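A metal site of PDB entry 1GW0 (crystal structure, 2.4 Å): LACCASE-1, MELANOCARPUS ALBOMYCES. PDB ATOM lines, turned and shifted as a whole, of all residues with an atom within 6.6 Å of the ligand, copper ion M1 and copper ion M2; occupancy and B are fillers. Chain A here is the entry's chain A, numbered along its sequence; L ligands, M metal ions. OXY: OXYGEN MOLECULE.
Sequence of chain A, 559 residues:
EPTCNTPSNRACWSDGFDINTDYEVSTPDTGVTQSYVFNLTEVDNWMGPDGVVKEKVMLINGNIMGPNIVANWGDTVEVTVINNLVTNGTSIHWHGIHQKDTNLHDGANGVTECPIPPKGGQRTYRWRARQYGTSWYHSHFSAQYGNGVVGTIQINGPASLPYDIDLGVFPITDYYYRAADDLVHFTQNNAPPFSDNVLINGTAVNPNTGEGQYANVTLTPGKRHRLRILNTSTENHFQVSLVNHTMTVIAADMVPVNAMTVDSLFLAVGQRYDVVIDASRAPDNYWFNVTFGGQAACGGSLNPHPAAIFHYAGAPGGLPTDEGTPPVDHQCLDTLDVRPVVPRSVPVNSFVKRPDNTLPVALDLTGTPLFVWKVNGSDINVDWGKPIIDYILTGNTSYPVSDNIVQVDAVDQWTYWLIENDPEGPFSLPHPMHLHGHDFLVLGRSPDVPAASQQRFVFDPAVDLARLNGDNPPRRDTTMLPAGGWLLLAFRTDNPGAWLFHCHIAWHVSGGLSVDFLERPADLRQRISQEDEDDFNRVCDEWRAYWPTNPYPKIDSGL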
ATOM      1  N   HIS A  93      -8.687  -8.392   1.074  1.00  0.00           N
ATOM      2  CA  HIS A  93      -7.271  -8.418   0.759  1.00  0.00           C
ATOM      3  C   HIS A  93      -6.789  -6.973   0.731  1.00  0.00           C
ATOM      4  O   HIS A  93      -7.499  -6.073   0.250  1.00  0.00           O
ATOM      5  CB  HIS A  93      -7.050  -9.098  -0.595  1.00  0.00           C
ATOM      6  CG  HIS A  93      -5.708  -8.811  -1.199  1.00  0.00           C
ATOM      7  ND1 HIS A  93      -4.522  -9.169  -0.582  1.00  0.00           N
ATOM      8  CD2 HIS A  93      -5.361  -8.169  -2.340  1.00  0.00           C
ATOM      9  CE1 HIS A  93      -3.509  -8.757  -1.322  1.00  0.00           C
ATOM     10  NE2 HIS A  93      -3.991  -8.151  -2.388  1.00  0.00           N
ATOM     11  N   TRP A  94      -5.591  -6.752   1.265  1.00  0.00           N
ATOM     12  CA  TRP A  94      -5.007  -5.426   1.344  1.00  0.00           C
ATOM     13  C   TRP A  94      -3.961  -5.274   0.245  1.00  0.00           C
ATOM     14  O   TRP A  94      -2.764  -5.490   0.457  1.00  0.00           O
ATOM     15  CB  TRP A  94      -4.408  -5.204   2.739  1.00  0.00           C
ATOM     16  CG  TRP A  94      -5.283  -5.780   3.826  1.00  0.00           C
ATOM     17  CD1 TRP A  94      -5.238  -7.058   4.326  1.00  0.00           C
ATOM     18  CD2 TRP A  94      -6.424  -5.152   4.427  1.00  0.00           C
ATOM     19  NE1 TRP A  94      -6.298  -7.265   5.177  1.00  0.00           N
ATOM     20  CE2 TRP A  94      -7.028  -6.113   5.267  1.00  0.00           C
ATOM     21  CE3 TRP A  94      -6.990  -3.876   4.336  1.00  0.00           C
ATOM     22  CZ2 TRP A  94      -8.189  -5.838   5.997  1.00  0.00           C
ATOM     23  CZ3 TRP A  94      -8.142  -3.603   5.064  1.00  0.00           C
ATOM     24  CH2 TRP A  94      -8.734  -4.582   5.883  1.00  0.00           C
ATOM     25  N   HIS A  95      -4.446  -4.912  -0.935  1.00  0.00           N
ATOM     26  CA  HIS A  95      -3.659  -4.738  -2.149  1.00  0.00           C
ATOM     27  C   HIS A  95      -2.516  -3.728  -2.008  1.00  0.00           C
ATOM     28  O   HIS A  95      -2.753  -2.523  -1.964  1.00  0.00           O
ATOM     29  CB  HIS A  95      -4.599  -4.301  -3.275  1.00  0.00           C
ATOM     30  CG  HIS A  95      -3.976  -4.351  -4.629  1.00  0.00           C
ATOM     31  ND1 HIS A  95      -4.397  -5.239  -5.608  1.00  0.00           N
ATOM     32  CD2 HIS A  95      -2.973  -3.638  -5.186  1.00  0.00           C
ATOM     33  CE1 HIS A  95      -3.679  -5.055  -6.695  1.00  0.00           C
ATOM     34  NE2 HIS A  95      -2.806  -4.085  -6.472  1.00  0.00           N
ATOM     35  N   GLY A  96      -1.282  -4.225  -1.967  1.00  0.00           N
ATOM     36  CA  GLY A  96      -0.145  -3.339  -1.840  1.00  0.00           C
ATOM     37  C   GLY A  96       0.592  -3.552  -0.532  1.00  0.00           C
ATOM     38  O   GLY A  96       1.760  -3.190  -0.396  1.00  0.00           O
ATOM     39  N   ASP A 106      -3.400 -11.816   4.823  1.00  0.00           N
ATOM     40  CA  ASP A 106      -3.414 -11.342   3.439  1.00  0.00           C
ATOM     41  C   ASP A 106      -4.813 -11.259   2.845  1.00  0.00           C
ATOM     42  O   ASP A 106      -5.066 -10.454   1.942  1.00  0.00           O
ATOM     43  CB  ASP A 106      -2.527 -12.242   2.554  1.00  0.00           C
ATOM     44  CG  ASP A 106      -2.325 -11.673   1.163  1.00  0.00           C
ATOM     45  OD1 ASP A 106      -1.914 -10.498   1.056  1.00  0.00           O
ATOM     46  OD2 ASP A 106      -2.559 -12.406   0.185  1.00  0.00           O
ATOM     47  N   ALA A 108      -6.567 -13.804   1.273  1.00  0.00           N
ATOM     48  CA  ALA A 108      -6.709 -14.590   0.049  1.00  0.00           C
ATOM     49  C   ALA A 108      -7.491 -15.862   0.367  1.00  0.00           C
ATOM     50  O   ALA A 108      -6.892 -16.893   0.645  1.00  0.00           O
ATOM     51  CB  ALA A 108      -5.328 -14.937  -0.481  1.00  0.00           C
ATOM     52  N   TRP A 136      -4.965   0.134  -1.694  1.00  0.00           N
ATOM     53  CA  TRP A 136      -6.398  -0.056  -1.569  1.00  0.00           C
ATOM     54  C   TRP A 136      -6.726  -1.468  -1.111  1.00  0.00           C
ATOM     55  O   TRP A 136      -5.837  -2.321  -1.052  1.00  0.00           O
ATOM     56  CB  TRP A 136      -7.083   0.250  -2.906  1.00  0.00           C
ATOM     57  CG  TRP A 136      -6.661  -0.647  -4.068  1.00  0.00           C
ATOM     58  CD1 TRP A 136      -5.381  -0.876  -4.510  1.00  0.00           C
ATOM     59  CD2 TRP A 136      -7.522  -1.408  -4.932  1.00  0.00           C
ATOM     60  NE1 TRP A 136      -5.404  -1.729  -5.599  1.00  0.00           N
ATOM     61  CE2 TRP A 136      -6.699  -2.064  -5.873  1.00  0.00           C
ATOM     62  CE3 TRP A 136      -8.920  -1.588  -4.995  1.00  0.00           C
ATOM     63  CZ2 TRP A 136      -7.229  -2.896  -6.864  1.00  0.00           C
ATOM     64  CZ3 TRP A 136      -9.439  -2.410  -5.994  1.00  0.00           C
ATOM     65  CH2 TRP A 136      -8.589  -3.058  -6.916  1.00  0.00           C
ATOM     66  N   TYR A 137      -7.987  -1.722  -0.772  1.00  0.00           N
ATOM     67  CA  TYR A 137      -8.376  -3.048  -0.324  1.00  0.00           C
ATOM     68  C   TYR A 137      -9.651  -3.442  -1.029  1.00  0.00           C
ATOM     69  O   TYR A 137     -10.414  -2.580  -1.481  1.00  0.00           O
ATOM     70  CB  TYR A 137      -8.580  -3.095   1.203  1.00  0.00           C
ATOM     71  CG  TYR A 137      -9.573  -2.083   1.738  1.00  0.00           C
ATOM     72  CD1 TYR A 137      -9.168  -0.807   2.118  1.00  0.00           C
ATOM     73  CD2 TYR A 137     -10.928  -2.397   1.811  1.00  0.00           C
ATOM     74  CE1 TYR A 137     -10.102   0.156   2.557  1.00  0.00           C
ATOM     75  CE2 TYR A 137     -11.867  -1.466   2.250  1.00  0.00           C
ATOM     76  CZ  TYR A 137     -11.445  -0.189   2.615  1.00  0.00           C
ATOM     77  OH  TYR A 137     -12.398   0.725   3.017  1.00  0.00           O
ATOM     78  N   HIS A 138      -9.878  -4.741  -1.126  1.00  0.00           N
ATOM     79  CA  HIS A 138     -11.069  -5.247  -1.793  1.00  0.00           C
ATOM     80  C   HIS A 138     -11.285  -6.712  -1.466  1.00  0.00           C
ATOM     81  O   HIS A 138     -10.381  -7.401  -0.997  1.00  0.00           O
ATOM     82  CB  HIS A 138     -10.932  -5.078  -3.304  1.00  0.00           C
ATOM     83  CG  HIS A 138      -9.701  -5.707  -3.880  1.00  0.00           C
ATOM     84  ND1 HIS A 138      -9.561  -7.071  -4.021  1.00  0.00           N
ATOM     85  CD2 HIS A 138      -8.539  -5.165  -4.317  1.00  0.00           C
ATOM     86  CE1 HIS A 138      -8.370  -7.342  -4.527  1.00  0.00           C
ATOM     87  NE2 HIS A 138      -7.727  -6.201  -4.727  1.00  0.00           N
ATOM     88  N   SER A 139     -12.502  -7.190  -1.702  1.00  0.00           N
ATOM     89  CA  SER A 139     -12.823  -8.587  -1.459  1.00  0.00           C
ATOM     90  C   SER A 139     -12.056  -9.445  -2.467  1.00  0.00           C
ATOM     91  O   SER A 139     -11.658  -8.958  -3.547  1.00  0.00           O
ATOM     92  CB  SER A 139     -14.324  -8.810  -1.638  1.00  0.00           C
ATOM     93  OG  SER A 139     -14.655 -10.170  -1.498  1.00  0.00           O
ATOM     94  N   HIS A 140     -11.829 -10.713  -2.119  1.00  0.00           N
ATOM     95  CA  HIS A 140     -11.139 -11.643  -3.009  1.00  0.00           C
ATOM     96  C   HIS A 140     -12.039 -12.872  -3.152  1.00  0.00           C
ATOM     97  O   HIS A 140     -11.608 -13.905  -3.649  1.00  0.00           O
ATOM     98  CB  HIS A 140      -9.766 -12.046  -2.447  1.00  0.00           C
ATOM     99  CG  HIS A 140      -8.655 -12.006  -3.460  1.00  0.00           C
ATOM    100  ND1 HIS A 140      -8.765 -12.573  -4.715  1.00  0.00           N
ATOM    101  CD2 HIS A 140      -7.409 -11.456  -3.398  1.00  0.00           C
ATOM    102  CE1 HIS A 140      -7.646 -12.363  -5.392  1.00  0.00           C
ATOM    103  NE2 HIS A 140      -6.805 -11.686  -4.622  1.00  0.00           N
ATOM    104  N   TYR A 145     -15.931  -7.927  -5.098  1.00  0.00           N
ATOM    105  CA  TYR A 145     -15.589  -6.520  -4.960  1.00  0.00           C
ATOM    106  C   TYR A 145     -16.150  -5.687  -6.086  1.00  0.00           C
ATOM    107  O   TYR A 145     -16.069  -4.470  -6.079  1.00  0.00           O
ATOM    108  CB  TYR A 145     -14.062  -6.338  -4.813  1.00  0.00           C
ATOM    109  CG  TYR A 145     -13.233  -6.095  -6.073  1.00  0.00           C
ATOM    110  CD1 TYR A 145     -13.212  -4.848  -6.697  1.00  0.00           C
ATOM    111  CD2 TYR A 145     -12.420  -7.099  -6.580  1.00  0.00           C
ATOM    112  CE1 TYR A 145     -12.380  -4.605  -7.794  1.00  0.00           C
ATOM    113  CE2 TYR A 145     -11.583  -6.880  -7.677  1.00  0.00           C
ATOM    114  CZ  TYR A 145     -11.565  -5.629  -8.277  1.00  0.00           C
ATOM    115  OH  TYR A 145     -10.722  -5.421  -9.346  1.00  0.00           O
ATOM    116  N   GLY A 270      -5.762  -1.868 -10.696  1.00  0.00           N
ATOM    117  CA  GLY A 270      -4.983  -2.063  -9.476  1.00  0.00           C
ATOM    118  C   GLY A 270      -3.772  -1.155  -9.247  1.00  0.00           C
ATOM    119  O   GLY A 270      -3.191  -1.195  -8.168  1.00  0.00           O
ATOM    120  N   HIS A 434      -0.537  -9.084 -11.160  1.00  0.00           N
ATOM    121  CA  HIS A 434      -0.329  -8.603  -9.794  1.00  0.00           C
ATOM    122  C   HIS A 434       0.170  -9.689  -8.841  1.00  0.00           C
ATOM    123  O   HIS A 434      -0.271 -10.832  -8.868  1.00  0.00           O
ATOM    124  CB  HIS A 434      -1.646  -8.007  -9.278  1.00  0.00           C
ATOM    125  CG  HIS A 434      -1.677  -7.793  -7.794  1.00  0.00           C
ATOM    126  ND1 HIS A 434      -0.869  -6.878  -7.154  1.00  0.00           N
ATOM    127  CD2 HIS A 434      -2.402  -8.403  -6.827  1.00  0.00           C
ATOM    128  CE1 HIS A 434      -1.106  -6.926  -5.860  1.00  0.00           C
ATOM    129  NE2 HIS A 434      -2.023  -7.839  -5.626  1.00  0.00           N
ATOM    130  N   HIS A 436       0.928 -10.757  -4.738  1.00  0.00           N
ATOM    131  CA  HIS A 436       0.693 -10.519  -3.323  1.00  0.00           C
ATOM    132  C   HIS A 436       2.040 -10.727  -2.603  1.00  0.00           C
ATOM    133  O   HIS A 436       2.908 -11.458  -3.092  1.00  0.00           O
ATOM    134  CB  HIS A 436      -0.302 -11.530  -2.730  1.00  0.00           C
ATOM    135  CG  HIS A 436      -1.723 -11.365  -3.189  1.00  0.00           C
ATOM    136  ND1 HIS A 436      -2.788 -11.893  -2.483  1.00  0.00           N
ATOM    137  CD2 HIS A 436      -2.256 -10.795  -4.302  1.00  0.00           C
ATOM    138  CE1 HIS A 436      -3.914 -11.656  -3.148  1.00  0.00           C
ATOM    139  NE2 HIS A 436      -3.616 -10.992  -4.249  1.00  0.00           N
ATOM    140  N   LEU A 500      -0.513 -15.323  -3.925  1.00  0.00           N
ATOM    141  CA  LEU A 500      -1.151 -15.379  -5.227  1.00  0.00           C
ATOM    142  C   LEU A 500      -0.459 -14.406  -6.177  1.00  0.00           C
ATOM    143  O   LEU A 500       0.059 -13.344  -5.772  1.00  0.00           O
ATOM    144  CB  LEU A 500      -2.633 -15.017  -5.118  1.00  0.00           C
ATOM    145  CG  LEU A 500      -3.570 -16.070  -4.510  1.00  0.00           C
ATOM    146  CD1 LEU A 500      -4.946 -15.476  -4.365  1.00  0.00           C
ATOM    147  CD2 LEU A 500      -3.616 -17.317  -5.375  1.00  0.00           C
ATOM    148  N   PHE A 501      -0.430 -14.805  -7.461  1.00  0.00           N
ATOM    149  CA  PHE A 501       0.137 -14.024  -8.548  1.00  0.00           C
ATOM    150  C   PHE A 501      -0.915 -14.232  -9.640  1.00  0.00           C
ATOM    151  O   PHE A 501      -0.952 -15.278 -10.299  1.00  0.00           O
ATOM    152  CB  PHE A 501       1.499 -14.577  -8.968  1.00  0.00           C
ATOM    153  CG  PHE A 501       2.125 -13.836 -10.115  1.00  0.00           C
ATOM    154  CD1 PHE A 501       2.339 -12.461 -10.041  1.00  0.00           C
ATOM    155  CD2 PHE A 501       2.466 -14.493 -11.277  1.00  0.00           C
ATOM    156  CE1 PHE A 501       2.874 -11.751 -11.116  1.00  0.00           C
ATOM    157  CE2 PHE A 501       3.015 -13.805 -12.364  1.00  0.00           C
ATOM    158  CZ  PHE A 501       3.210 -12.426 -12.284  1.00  0.00           C
ATOM    159  N   HIS A 502      -1.772 -13.246  -9.829  1.00  0.00           N
ATOM    160  CA  HIS A 502      -2.855 -13.371 -10.784  1.00  0.00           C
ATOM    161  C   HIS A 502      -3.070 -12.145 -11.641  1.00  0.00           C
ATOM    162  O   HIS A 502      -2.409 -11.126 -11.456  1.00  0.00           O
ATOM    163  CB  HIS A 502      -4.142 -13.703 -10.023  1.00  0.00           C
ATOM    164  CG  HIS A 502      -4.538 -12.679  -9.003  1.00  0.00           C
ATOM    165  ND1 HIS A 502      -5.208 -11.516  -9.325  1.00  0.00           N
ATOM    166  CD2 HIS A 502      -4.353 -12.631  -7.658  1.00  0.00           C
ATOM    167  CE1 HIS A 502      -5.424 -10.815  -8.236  1.00  0.00           C
ATOM    168  NE2 HIS A 502      -4.916 -11.461  -7.202  1.00  0.00           N
ATOM    169  N   HIS A 504      -5.389  -9.103 -12.576  1.00  0.00           N
ATOM    170  CA  HIS A 504      -6.401  -8.399 -11.785  1.00  0.00           C
ATOM    171  C   HIS A 504      -7.723  -8.099 -12.474  1.00  0.00           C
ATOM    172  O   HIS A 504      -8.570  -7.420 -11.912  1.00  0.00           O
ATOM    173  CB  HIS A 504      -5.822  -7.110 -11.195  1.00  0.00           C
ATOM    174  CG  HIS A 504      -6.254  -6.860  -9.780  1.00  0.00           C
ATOM    175  ND1 HIS A 504      -7.563  -6.591  -9.436  1.00  0.00           N
ATOM    176  CD2 HIS A 504      -5.548  -6.852  -8.620  1.00  0.00           C
ATOM    177  CE1 HIS A 504      -7.640  -6.427  -8.125  1.00  0.00           C
ATOM    178  NE2 HIS A 504      -6.443  -6.581  -7.606  1.00  0.00           N
ATOM    179  N   VAL A 509      -9.209 -13.739 -13.574  1.00  0.00           N
ATOM    180  CA  VAL A 509      -8.785 -14.489 -12.389  1.00  0.00           C
ATOM    181  C   VAL A 509      -9.920 -15.448 -12.031  1.00  0.00           C
ATOM    182  O   VAL A 509      -9.698 -16.589 -11.634  1.00  0.00           O
ATOM    183  CB  VAL A 509      -8.514 -13.547 -11.184  1.00  0.00           C
ATOM    184  CG1 VAL A 509      -9.828 -12.958 -10.650  1.00  0.00           C
ATOM    185  CG2 VAL A 509      -7.757 -14.291 -10.096  1.00  0.00           C
ATOM    186  N   LEU A 559     -11.440 -17.018  -6.784  1.00  0.00           N
ATOM    187  CA  LEU A 559     -10.547 -15.875  -6.607  1.00  0.00           C
ATOM    188  C   LEU A 559     -11.005 -14.613  -7.337  1.00  0.00           C
ATOM    189  O   LEU A 559     -10.521 -13.519  -6.967  1.00  0.00           O
ATOM    190  CB  LEU A 559      -9.122 -16.243  -7.078  1.00  0.00           C
ATOM    191  CG  LEU A 559      -8.442 -17.382  -6.313  1.00  0.00           C
ATOM    192  CD1 LEU A 559      -6.979 -17.517  -6.766  1.00  0.00           C
ATOM    193  CD2 LEU A 559      -8.509 -17.098  -4.815  1.00  0.00           C
ATOM    194  OXT LEU A 559     -11.836 -14.730  -8.263  1.00  0.00           O
HETATM  195  O1  OXY L   1      -5.065  -8.282  -5.398  1.00  0.00           O
HETATM  196  O2  OXY L   1      -6.146  -8.719  -5.744  1.00  0.00           O
HETATM  197 CU    CU M   1      -6.107  -6.056  -5.758  1.00  0.00          CU
HETATM  198 CU    CU M   2      -5.187 -10.868  -5.349  1.00  0.00          CU
HETATM  199 CU    CU M   3      -2.921  -7.998  -3.938  1.00  0.00          CU
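The backbone carbonyl oxygen of Gly 270 is in hydrogen-bond range of a ring nitrogen (NE2) of His 95, at 3.4 Å.
The backbone NH (N) of His 436 is in hydrogen-bond range of the backbone carbonyl oxygen (O) of Leu 500, 2.9 Å away.
A ring nitrogen (ND1) of His 436 is in hydrogen-bond range of the side-chain carboxylate (OD2) of Asp 106 (2.7 Å).
A ring nitrogen (ND1) of His 504 sits at hydrogen-bond distance from the side-chain hydroxyl (OH) of Tyr 145 (3.4 Å).
The chain-end carboxylate (O) of Leu 559 lies within hydrogen-bond range of a ring nitrogen (ND1) of His 140, 3.0 Å away.
The backbone carbonyl oxygen (O) of His 502 is in hydrogen-bond range of the backbone NH (N) of His 434 (2.8 Å).
A ring nitrogen (ND1) of His 93 sits at hydrogen-bond distance from the backbone carbonyl oxygen (O) of Asp 106 (2.9 Å).
NE1 of Trp 136 sits at hydrogen-bond distance from O of Gly 270, at 3.4 Å.
NE2 of His 436 is bound to copper ion M2 (1.9 Å).
NE2 of His 140 binds copper ion M2 (2.0 Å).
NE2 of His 502 is bound to copper ion M2, 2.0 Å away.
O2 of the ligand is bound to copper ion M2 (2.4 Å).
Residues that only touch copper ion M1: Trp 136.
Within 4 Å of copper ion M1: His 95, Trp 136, His 138 and His 504.
The nearest printed residue that does not touch copper ion M1 is His 93 (4.1 Å).
A ring nitrogen (NE2) of His 93 sits close to an oxygen (O1) of the ligand (3.2 Å).
An oxygen (O1) of the ligand sits close to a ring nitrogen (NE2) of His 434 (3.1 Å).
Hydrophobic or aromatic side chains that line the ligand: His 93, His 95, His 138, His 140, His 434, His 436, His 502 and His 504.
The nearest printed residue that does not touch the ligand is Ser 139 (5.9 Å).
Copper ion M1 is bound by ND1 of His 95 (1.9 Å), NE2 of His 138 (1.9 Å), NE2 of His 504 (2.0 Å) and O1 of the ligand (2.5 Å).
Copper ion M1 has four donor atoms within binding distance.
Along chain A the residues within 4 Å of copper ion M2 span positions 140 to 502.
The nearest printed residue that does not touch copper ion M2 is His 434 (4.002 Å).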
